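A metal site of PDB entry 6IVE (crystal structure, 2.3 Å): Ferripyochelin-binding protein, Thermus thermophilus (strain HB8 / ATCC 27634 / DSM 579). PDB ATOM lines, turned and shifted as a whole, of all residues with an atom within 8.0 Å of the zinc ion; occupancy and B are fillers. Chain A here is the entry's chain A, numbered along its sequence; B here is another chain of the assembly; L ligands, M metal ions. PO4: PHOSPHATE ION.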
ATOM      1  N   ARG A  46      -9.509 -19.776 -19.777  1.00  0.00           N
ATOM      2  CA  ARG A  46     -10.446 -18.714 -20.102  1.00  0.00           C
ATOM      3  C   ARG A  46      -9.850 -17.792 -21.144  1.00  0.00           C
ATOM      4  O   ARG A  46      -8.740 -17.287 -20.975  1.00  0.00           O
ATOM      5  CB  ARG A  46     -10.831 -17.915 -18.843  1.00  0.00           C
ATOM      6  CG  ARG A  46     -11.718 -16.707 -19.099  1.00  0.00           C
ATOM      7  CD  ARG A  46     -12.515 -16.330 -17.862  1.00  0.00           C
ATOM      8  NE  ARG A  46     -11.662 -15.931 -16.737  1.00  0.00           N
ATOM      9  CZ  ARG A  46     -11.232 -14.688 -16.525  1.00  0.00           C
ATOM     10  NH1 ARG A  46     -11.573 -13.714 -17.358  1.00  0.00           N
ATOM     11  NH2 ARG A  46     -10.470 -14.425 -15.470  1.00  0.00           N
ATOM     12  N   ASP A  48     -11.222 -14.446 -23.223  1.00  0.00           N
ATOM     13  CA  ASP A  48     -12.284 -13.481 -23.513  1.00  0.00           C
ATOM     14  C   ASP A  48     -11.717 -12.232 -24.171  1.00  0.00           C
ATOM     15  O   ASP A  48     -12.012 -11.951 -25.332  1.00  0.00           O
ATOM     16  CB  ASP A  48     -13.055 -13.140 -22.228  1.00  0.00           C
ATOM     17  CG  ASP A  48     -12.160 -13.083 -21.001  1.00  0.00           C
ATOM     18  OD1 ASP A  48     -11.125 -12.378 -21.041  1.00  0.00           O
ATOM     19  OD2 ASP A  48     -12.498 -13.738 -19.995  1.00  0.00           O
ATOM     20  N   VAL A  65      -4.247 -22.328 -14.166  1.00  0.00           N
ATOM     21  CA  VAL A  65      -5.051 -21.251 -14.741  1.00  0.00           C
ATOM     22  C   VAL A  65      -4.347 -20.740 -15.990  1.00  0.00           C
ATOM     23  O   VAL A  65      -3.151 -20.406 -15.952  1.00  0.00           O
ATOM     24  CB  VAL A  65      -5.265 -20.098 -13.736  1.00  0.00           C
ATOM     25  CG1 VAL A  65      -5.975 -18.924 -14.429  1.00  0.00           C
ATOM     26  CG2 VAL A  65      -6.080 -20.568 -12.542  1.00  0.00           C
ATOM     27  N   LEU A  66      -5.079 -20.690 -17.104  1.00  0.00           N
ATOM     28  CA  LEU A  66      -4.628 -20.037 -18.323  1.00  0.00           C
ATOM     29  C   LEU A  66      -5.503 -18.810 -18.576  1.00  0.00           C
ATOM     30  O   LEU A  66      -6.739 -18.896 -18.477  1.00  0.00           O
ATOM     31  CB  LEU A  66      -4.713 -20.981 -19.525  1.00  0.00           C
ATOM     32  CG  LEU A  66      -3.905 -22.278 -19.503  1.00  0.00           C
ATOM     33  CD1 LEU A  66      -3.969 -22.941 -20.873  1.00  0.00           C
ATOM     34  CD2 LEU A  66      -2.463 -22.021 -19.110  1.00  0.00           C
ATOM     35  N   HIS A  67      -4.868 -17.692 -18.903  1.00  0.00           N
ATOM     36  CA  HIS A  67      -5.597 -16.498 -19.310  1.00  0.00           C
ATOM     37  C   HIS A  67      -4.677 -15.677 -20.206  1.00  0.00           C
ATOM     38  O   HIS A  67      -3.504 -15.995 -20.395  1.00  0.00           O
ATOM     39  CB  HIS A  67      -6.081 -15.699 -18.100  1.00  0.00           C
ATOM     40  CG  HIS A  67      -7.092 -14.647 -18.443  1.00  0.00           C
ATOM     41  ND1 HIS A  67      -7.085 -13.391 -17.880  1.00  0.00           N
ATOM     42  CD2 HIS A  67      -8.147 -14.678 -19.295  1.00  0.00           C
ATOM     43  CE1 HIS A  67      -8.099 -12.688 -18.369  1.00  0.00           C
ATOM     44  NE2 HIS A  67      -8.754 -13.440 -19.226  1.00  0.00           N
ATOM     45  N   ALA A  68      -5.228 -14.604 -20.769  1.00  0.00           N
ATOM     46  CA  ALA A  68      -4.491 -13.768 -21.700  1.00  0.00           C
ATOM     47  C   ALA A  68      -4.999 -12.334 -21.612  1.00  0.00           C
ATOM     48  O   ALA A  68      -6.166 -12.087 -21.282  1.00  0.00           O
ATOM     49  CB  ALA A  68      -4.622 -14.288 -23.134  1.00  0.00           C
ATOM     50  N   ASP A  69      -4.113 -11.391 -21.914  1.00  0.00           N
ATOM     51  CA  ASP A  69      -4.417  -9.972 -22.024  1.00  0.00           C
ATOM     52  C   ASP A  69      -4.355  -9.526 -23.473  1.00  0.00           C
ATOM     53  O   ASP A  69      -3.724 -10.196 -24.303  1.00  0.00           O
ATOM     54  CB  ASP A  69      -3.432  -9.147 -21.187  1.00  0.00           C
ATOM     55  CG  ASP A  69      -3.764  -9.161 -19.704  1.00  0.00           C
ATOM     56  OD1 ASP A  69      -4.920  -9.483 -19.361  1.00  0.00           O
ATOM     57  OD2 ASP A  69      -2.869  -8.847 -18.894  1.00  0.00           O
ATOM     58  N   VAL A  87       0.142 -20.854 -13.145  1.00  0.00           N
ATOM     59  CA  VAL A  87      -0.531 -19.774 -13.850  1.00  0.00           C
ATOM     60  C   VAL A  87       0.327 -19.408 -15.047  1.00  0.00           C
ATOM     61  O   VAL A  87       1.486 -19.013 -14.891  1.00  0.00           O
ATOM     62  CB  VAL A  87      -0.781 -18.552 -12.949  1.00  0.00           C
ATOM     63  CG1 VAL A  87      -1.580 -17.501 -13.710  1.00  0.00           C
ATOM     64  CG2 VAL A  87      -1.519 -18.978 -11.680  1.00  0.00           C
ATOM     65  N   VAL A  88      -0.233 -19.550 -16.237  1.00  0.00           N
ATOM     66  CA  VAL A  88       0.401 -19.122 -17.475  1.00  0.00           C
ATOM     67  C   VAL A  88      -0.482 -18.047 -18.067  1.00  0.00           C
ATOM     68  O   VAL A  88      -1.623 -18.323 -18.466  1.00  0.00           O
ATOM     69  CB  VAL A  88       0.612 -20.279 -18.450  1.00  0.00           C
ATOM     70  CG1 VAL A  88       1.399 -19.814 -19.668  1.00  0.00           C
ATOM     71  CG2 VAL A  88       1.312 -21.437 -17.755  1.00  0.00           C
ATOM     72  N   HIS A  89       0.018 -16.817 -18.114  1.00  0.00           N
ATOM     73  CA  HIS A  89      -0.795 -15.660 -18.463  1.00  0.00           C
ATOM     74  C   HIS A  89      -0.186 -14.942 -19.658  1.00  0.00           C
ATOM     75  O   HIS A  89       0.851 -14.288 -19.533  1.00  0.00           O
ATOM     76  CB  HIS A  89      -0.940 -14.708 -17.280  1.00  0.00           C
ATOM     77  CG  HIS A  89      -2.119 -13.802 -17.387  1.00  0.00           C
ATOM     78  ND1 HIS A  89      -2.150 -12.710 -18.225  1.00  0.00           N
ATOM     79  CD2 HIS A  89      -3.320 -13.832 -16.768  1.00  0.00           C
ATOM     80  CE1 HIS A  89      -3.313 -12.102 -18.112  1.00  0.00           C
ATOM     81  NE2 HIS A  89      -4.052 -12.767 -17.236  1.00  0.00           N
ATOM     82  N   GLY A  90      -0.827 -15.080 -20.814  1.00  0.00           N
ATOM     83  CA  GLY A  90      -0.446 -14.309 -21.990  1.00  0.00           C
ATOM     84  C   GLY A  90       0.964 -14.539 -22.459  1.00  0.00           C
ATOM     85  O   GLY A  90       1.610 -13.613 -22.957  1.00  0.00           O
ATOM     86  N   ASN A 107       2.847 -12.001 -18.671  1.00  0.00           N
ATOM     87  CA  ASN A 107       2.545 -11.609 -20.039  1.00  0.00           C
ATOM     88  C   ASN A 107       3.810 -11.409 -20.870  1.00  0.00           C
ATOM     89  O   ASN A 107       4.801 -10.843 -20.398  1.00  0.00           O
ATOM     90  CB  ASN A 107       1.720 -10.325 -20.055  1.00  0.00           C
ATOM     91  CG  ASN A 107       0.273 -10.541 -19.670  1.00  0.00           C
ATOM     92  OD1 ASN A 107      -0.255 -11.643 -19.778  1.00  0.00           O
ATOM     93  ND2 ASN A 107      -0.393  -9.473 -19.227  1.00  0.00           N
ATOM     94  N   GLN B  61     -10.329 -13.288  -9.000  1.00  0.00           N
ATOM     95  CA  GLN B  61     -10.153 -13.984 -10.261  1.00  0.00           C
ATOM     96  C   GLN B  61     -10.058 -15.501 -10.043  1.00  0.00           C
ATOM     97  O   GLN B  61     -10.196 -16.012  -8.926  1.00  0.00           O
ATOM     98  CB  GLN B  61      -8.927 -13.447 -10.992  1.00  0.00           C
ATOM     99  CG  GLN B  61      -9.076 -11.984 -11.376  1.00  0.00           C
ATOM    100  CD  GLN B  61      -7.870 -11.437 -12.107  1.00  0.00           C
ATOM    101  OE1 GLN B  61      -6.874 -12.132 -12.309  1.00  0.00           O
ATOM    102  NE2 GLN B  61      -7.959 -10.171 -12.527  1.00  0.00           N
ATOM    103  N   ASP B  62      -9.807 -16.213 -11.138  1.00  0.00           N
ATOM    104  CA  ASP B  62      -9.981 -17.665 -11.178  1.00  0.00           C
ATOM    105  C   ASP B  62      -9.044 -18.371 -10.208  1.00  0.00           C
ATOM    106  O   ASP B  62      -7.841 -18.104 -10.170  1.00  0.00           O
ATOM    107  CB  ASP B  62      -9.733 -18.180 -12.597  1.00  0.00           C
ATOM    108  CG  ASP B  62     -10.329 -17.267 -13.656  1.00  0.00           C
ATOM    109  OD1 ASP B  62      -9.719 -16.217 -13.935  1.00  0.00           O
ATOM    110  OD2 ASP B  62     -11.402 -17.602 -14.212  1.00  0.00           O
ATOM    111  N   GLY B  83      -5.741 -11.204  -8.221  1.00  0.00           N
ATOM    112  CA  GLY B  83      -5.361 -11.917  -9.427  1.00  0.00           C
ATOM    113  C   GLY B  83      -5.532 -13.417  -9.321  1.00  0.00           C
ATOM    114  O   GLY B  83      -5.740 -13.993  -8.251  1.00  0.00           O
ATOM    115  N   HIS B  84      -5.429 -14.062 -10.490  1.00  0.00           N
ATOM    116  CA  HIS B  84      -5.604 -15.508 -10.610  1.00  0.00           C
ATOM    117  C   HIS B  84      -4.796 -16.247  -9.545  1.00  0.00           C
ATOM    118  O   HIS B  84      -3.593 -16.015  -9.391  1.00  0.00           O
ATOM    119  CB  HIS B  84      -5.156 -15.991 -11.987  1.00  0.00           C
ATOM    120  CG  HIS B  84      -5.754 -15.239 -13.132  1.00  0.00           C
ATOM    121  ND1 HIS B  84      -7.057 -15.437 -13.564  1.00  0.00           N
ATOM    122  CD2 HIS B  84      -5.233 -14.303 -13.955  1.00  0.00           C
ATOM    123  CE1 HIS B  84      -7.296 -14.642 -14.589  1.00  0.00           C
ATOM    124  NE2 HIS B  84      -6.208 -13.954 -14.851  1.00  0.00           N
ATOM    125  N   MET B 101      -1.299 -12.096  -9.374  1.00  0.00           N
ATOM    126  CA  MET B 101      -1.682 -13.497  -9.496  1.00  0.00           C
ATOM    127  C   MET B 101      -0.662 -14.386  -8.792  1.00  0.00           C
ATOM    128  O   MET B 101       0.550 -14.172  -8.883  1.00  0.00           O
ATOM    129  CB  MET B 101      -1.822 -13.876 -10.970  1.00  0.00           C
ATOM    130  CG  MET B 101      -0.601 -13.592 -11.842  1.00  0.00           C
ATOM    131  SD  MET B 101      -0.962 -13.763 -13.609  1.00  0.00           S
ATOM    132  CE  MET B 101      -1.326 -12.075 -14.058  1.00  0.00           C
ATOM    133  N   ASN B 151      -7.027  -2.860 -13.646  1.00  0.00           N
ATOM    134  CA  ASN B 151      -7.736  -4.118 -13.856  1.00  0.00           C
ATOM    135  C   ASN B 151      -9.202  -4.015 -13.433  1.00  0.00           C
ATOM    136  O   ASN B 151     -10.082  -4.586 -14.089  1.00  0.00           O
ATOM    137  CB  ASN B 151      -7.048  -5.242 -13.086  1.00  0.00           C
ATOM    138  CG  ASN B 151      -5.551  -5.284 -13.314  1.00  0.00           C
ATOM    139  OD1 ASN B 151      -4.859  -4.265 -13.225  1.00  0.00           O
ATOM    140  ND2 ASN B 151      -5.035  -6.475 -13.627  1.00  0.00           N
ATOM    141  N   TYR B 155     -12.614  -5.414 -15.431  1.00  0.00           N
ATOM    142  CA  TYR B 155     -13.320  -6.583 -14.936  1.00  0.00           C
ATOM    143  C   TYR B 155     -14.759  -6.268 -14.538  1.00  0.00           C
ATOM    144  O   TYR B 155     -15.616  -7.145 -14.610  1.00  0.00           O
ATOM    145  CB  TYR B 155     -12.563  -7.198 -13.765  1.00  0.00           C
ATOM    146  CG  TYR B 155     -11.657  -8.324 -14.206  1.00  0.00           C
ATOM    147  CD1 TYR B 155     -10.391  -8.070 -14.713  1.00  0.00           C
ATOM    148  CD2 TYR B 155     -12.091  -9.645 -14.136  1.00  0.00           C
ATOM    149  CE1 TYR B 155      -9.573  -9.102 -15.126  1.00  0.00           C
ATOM    150  CE2 TYR B 155     -11.282 -10.682 -14.551  1.00  0.00           C
ATOM    151  CZ  TYR B 155     -10.019 -10.408 -15.045  1.00  0.00           C
ATOM    152  OH  TYR B 155      -9.215 -11.437 -15.459  1.00  0.00           O
ATOM    153  N   LEU B 158     -16.243  -6.704 -17.910  1.00  0.00           N
ATOM    154  CA  LEU B 158     -16.235  -8.110 -18.312  1.00  0.00           C
ATOM    155  C   LEU B 158     -17.241  -8.917 -17.513  1.00  0.00           C
ATOM    156  O   LEU B 158     -17.883  -9.824 -18.048  1.00  0.00           O
ATOM    157  CB  LEU B 158     -14.825  -8.679 -18.143  1.00  0.00           C
ATOM    158  CG  LEU B 158     -14.489  -9.995 -18.867  1.00  0.00           C
ATOM    159  CD1 LEU B 158     -14.569  -9.815 -20.380  1.00  0.00           C
ATOM    160  CD2 LEU B 158     -13.116 -10.505 -18.448  1.00  0.00           C
HETATM  161  P   PO4 L   1      -5.761  -9.692 -15.608  1.00  0.00           P
HETATM  162  O1  PO4 L   1      -4.372 -10.140 -15.228  1.00  0.00           O
HETATM  163  O2  PO4 L   1      -5.716  -8.811 -16.837  1.00  0.00           O
HETATM  164  O3  PO4 L   1      -6.359  -8.900 -14.470  1.00  0.00           O
HETATM  165  O4  PO4 L   1      -6.626 -10.889 -15.893  1.00  0.00           O
HETATM  166 ZN    ZN M   1      -5.810 -12.694 -16.366  1.00  0.00          ZN
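A ring nitrogen (ND1) of His 89 is in hydrogen-bond range of the side-chain amide oxygen (OD1) of Asn 107 (2.7 Å).
N of His 84 of chain B sits at hydrogen-bond distance from OE1 of Gln 61 of chain B, 3.0 Å away.
OD1 of Asp 62 of chain B is in hydrogen-bond range of ND1 of His 84 of chain B.
NE2 of His 67 lies within hydrogen-bond range of NH1 of Arg 46, at 3.4 Å.
A ring nitrogen (NE2) of His 67 sits at hydrogen-bond distance from the side-chain carboxylate of Asp 48, at 3.2 Å.
O of His 67 lies within hydrogen-bond range of N of Gly 90 (2.9 Å).
The side-chain amide nitrogen of Gln 61 of chain B sits close to the side-chain hydroxyl of Tyr 155 of chain B, 3.4 Å away.
The side-chain hydroxyl (OH) of Tyr 155 of chain B is in hydrogen-bond range of the guanidinium group (NH2) of Arg 46, at 3.2 Å.
Merely in contact with the zinc ion: Tyr 155 of chain B.
Of the 20 residues printed, 4 come within 4 Å of the zinc ion.
The nearest printed residue that does not touch the zinc ion is Gln 61 of chain B (4.2 Å).
The zinc ion is bound by a ring nitrogen (NE2) of His 89 (2.0 Å), a ring nitrogen (NE2) of His 84 of chain B (2.0 Å), an oxygen (O4) of the ligand (2.0 Å) and a ring nitrogen (ND1) of His 67 (2.1 Å).
The zinc ion has four donor atoms within binding distance.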
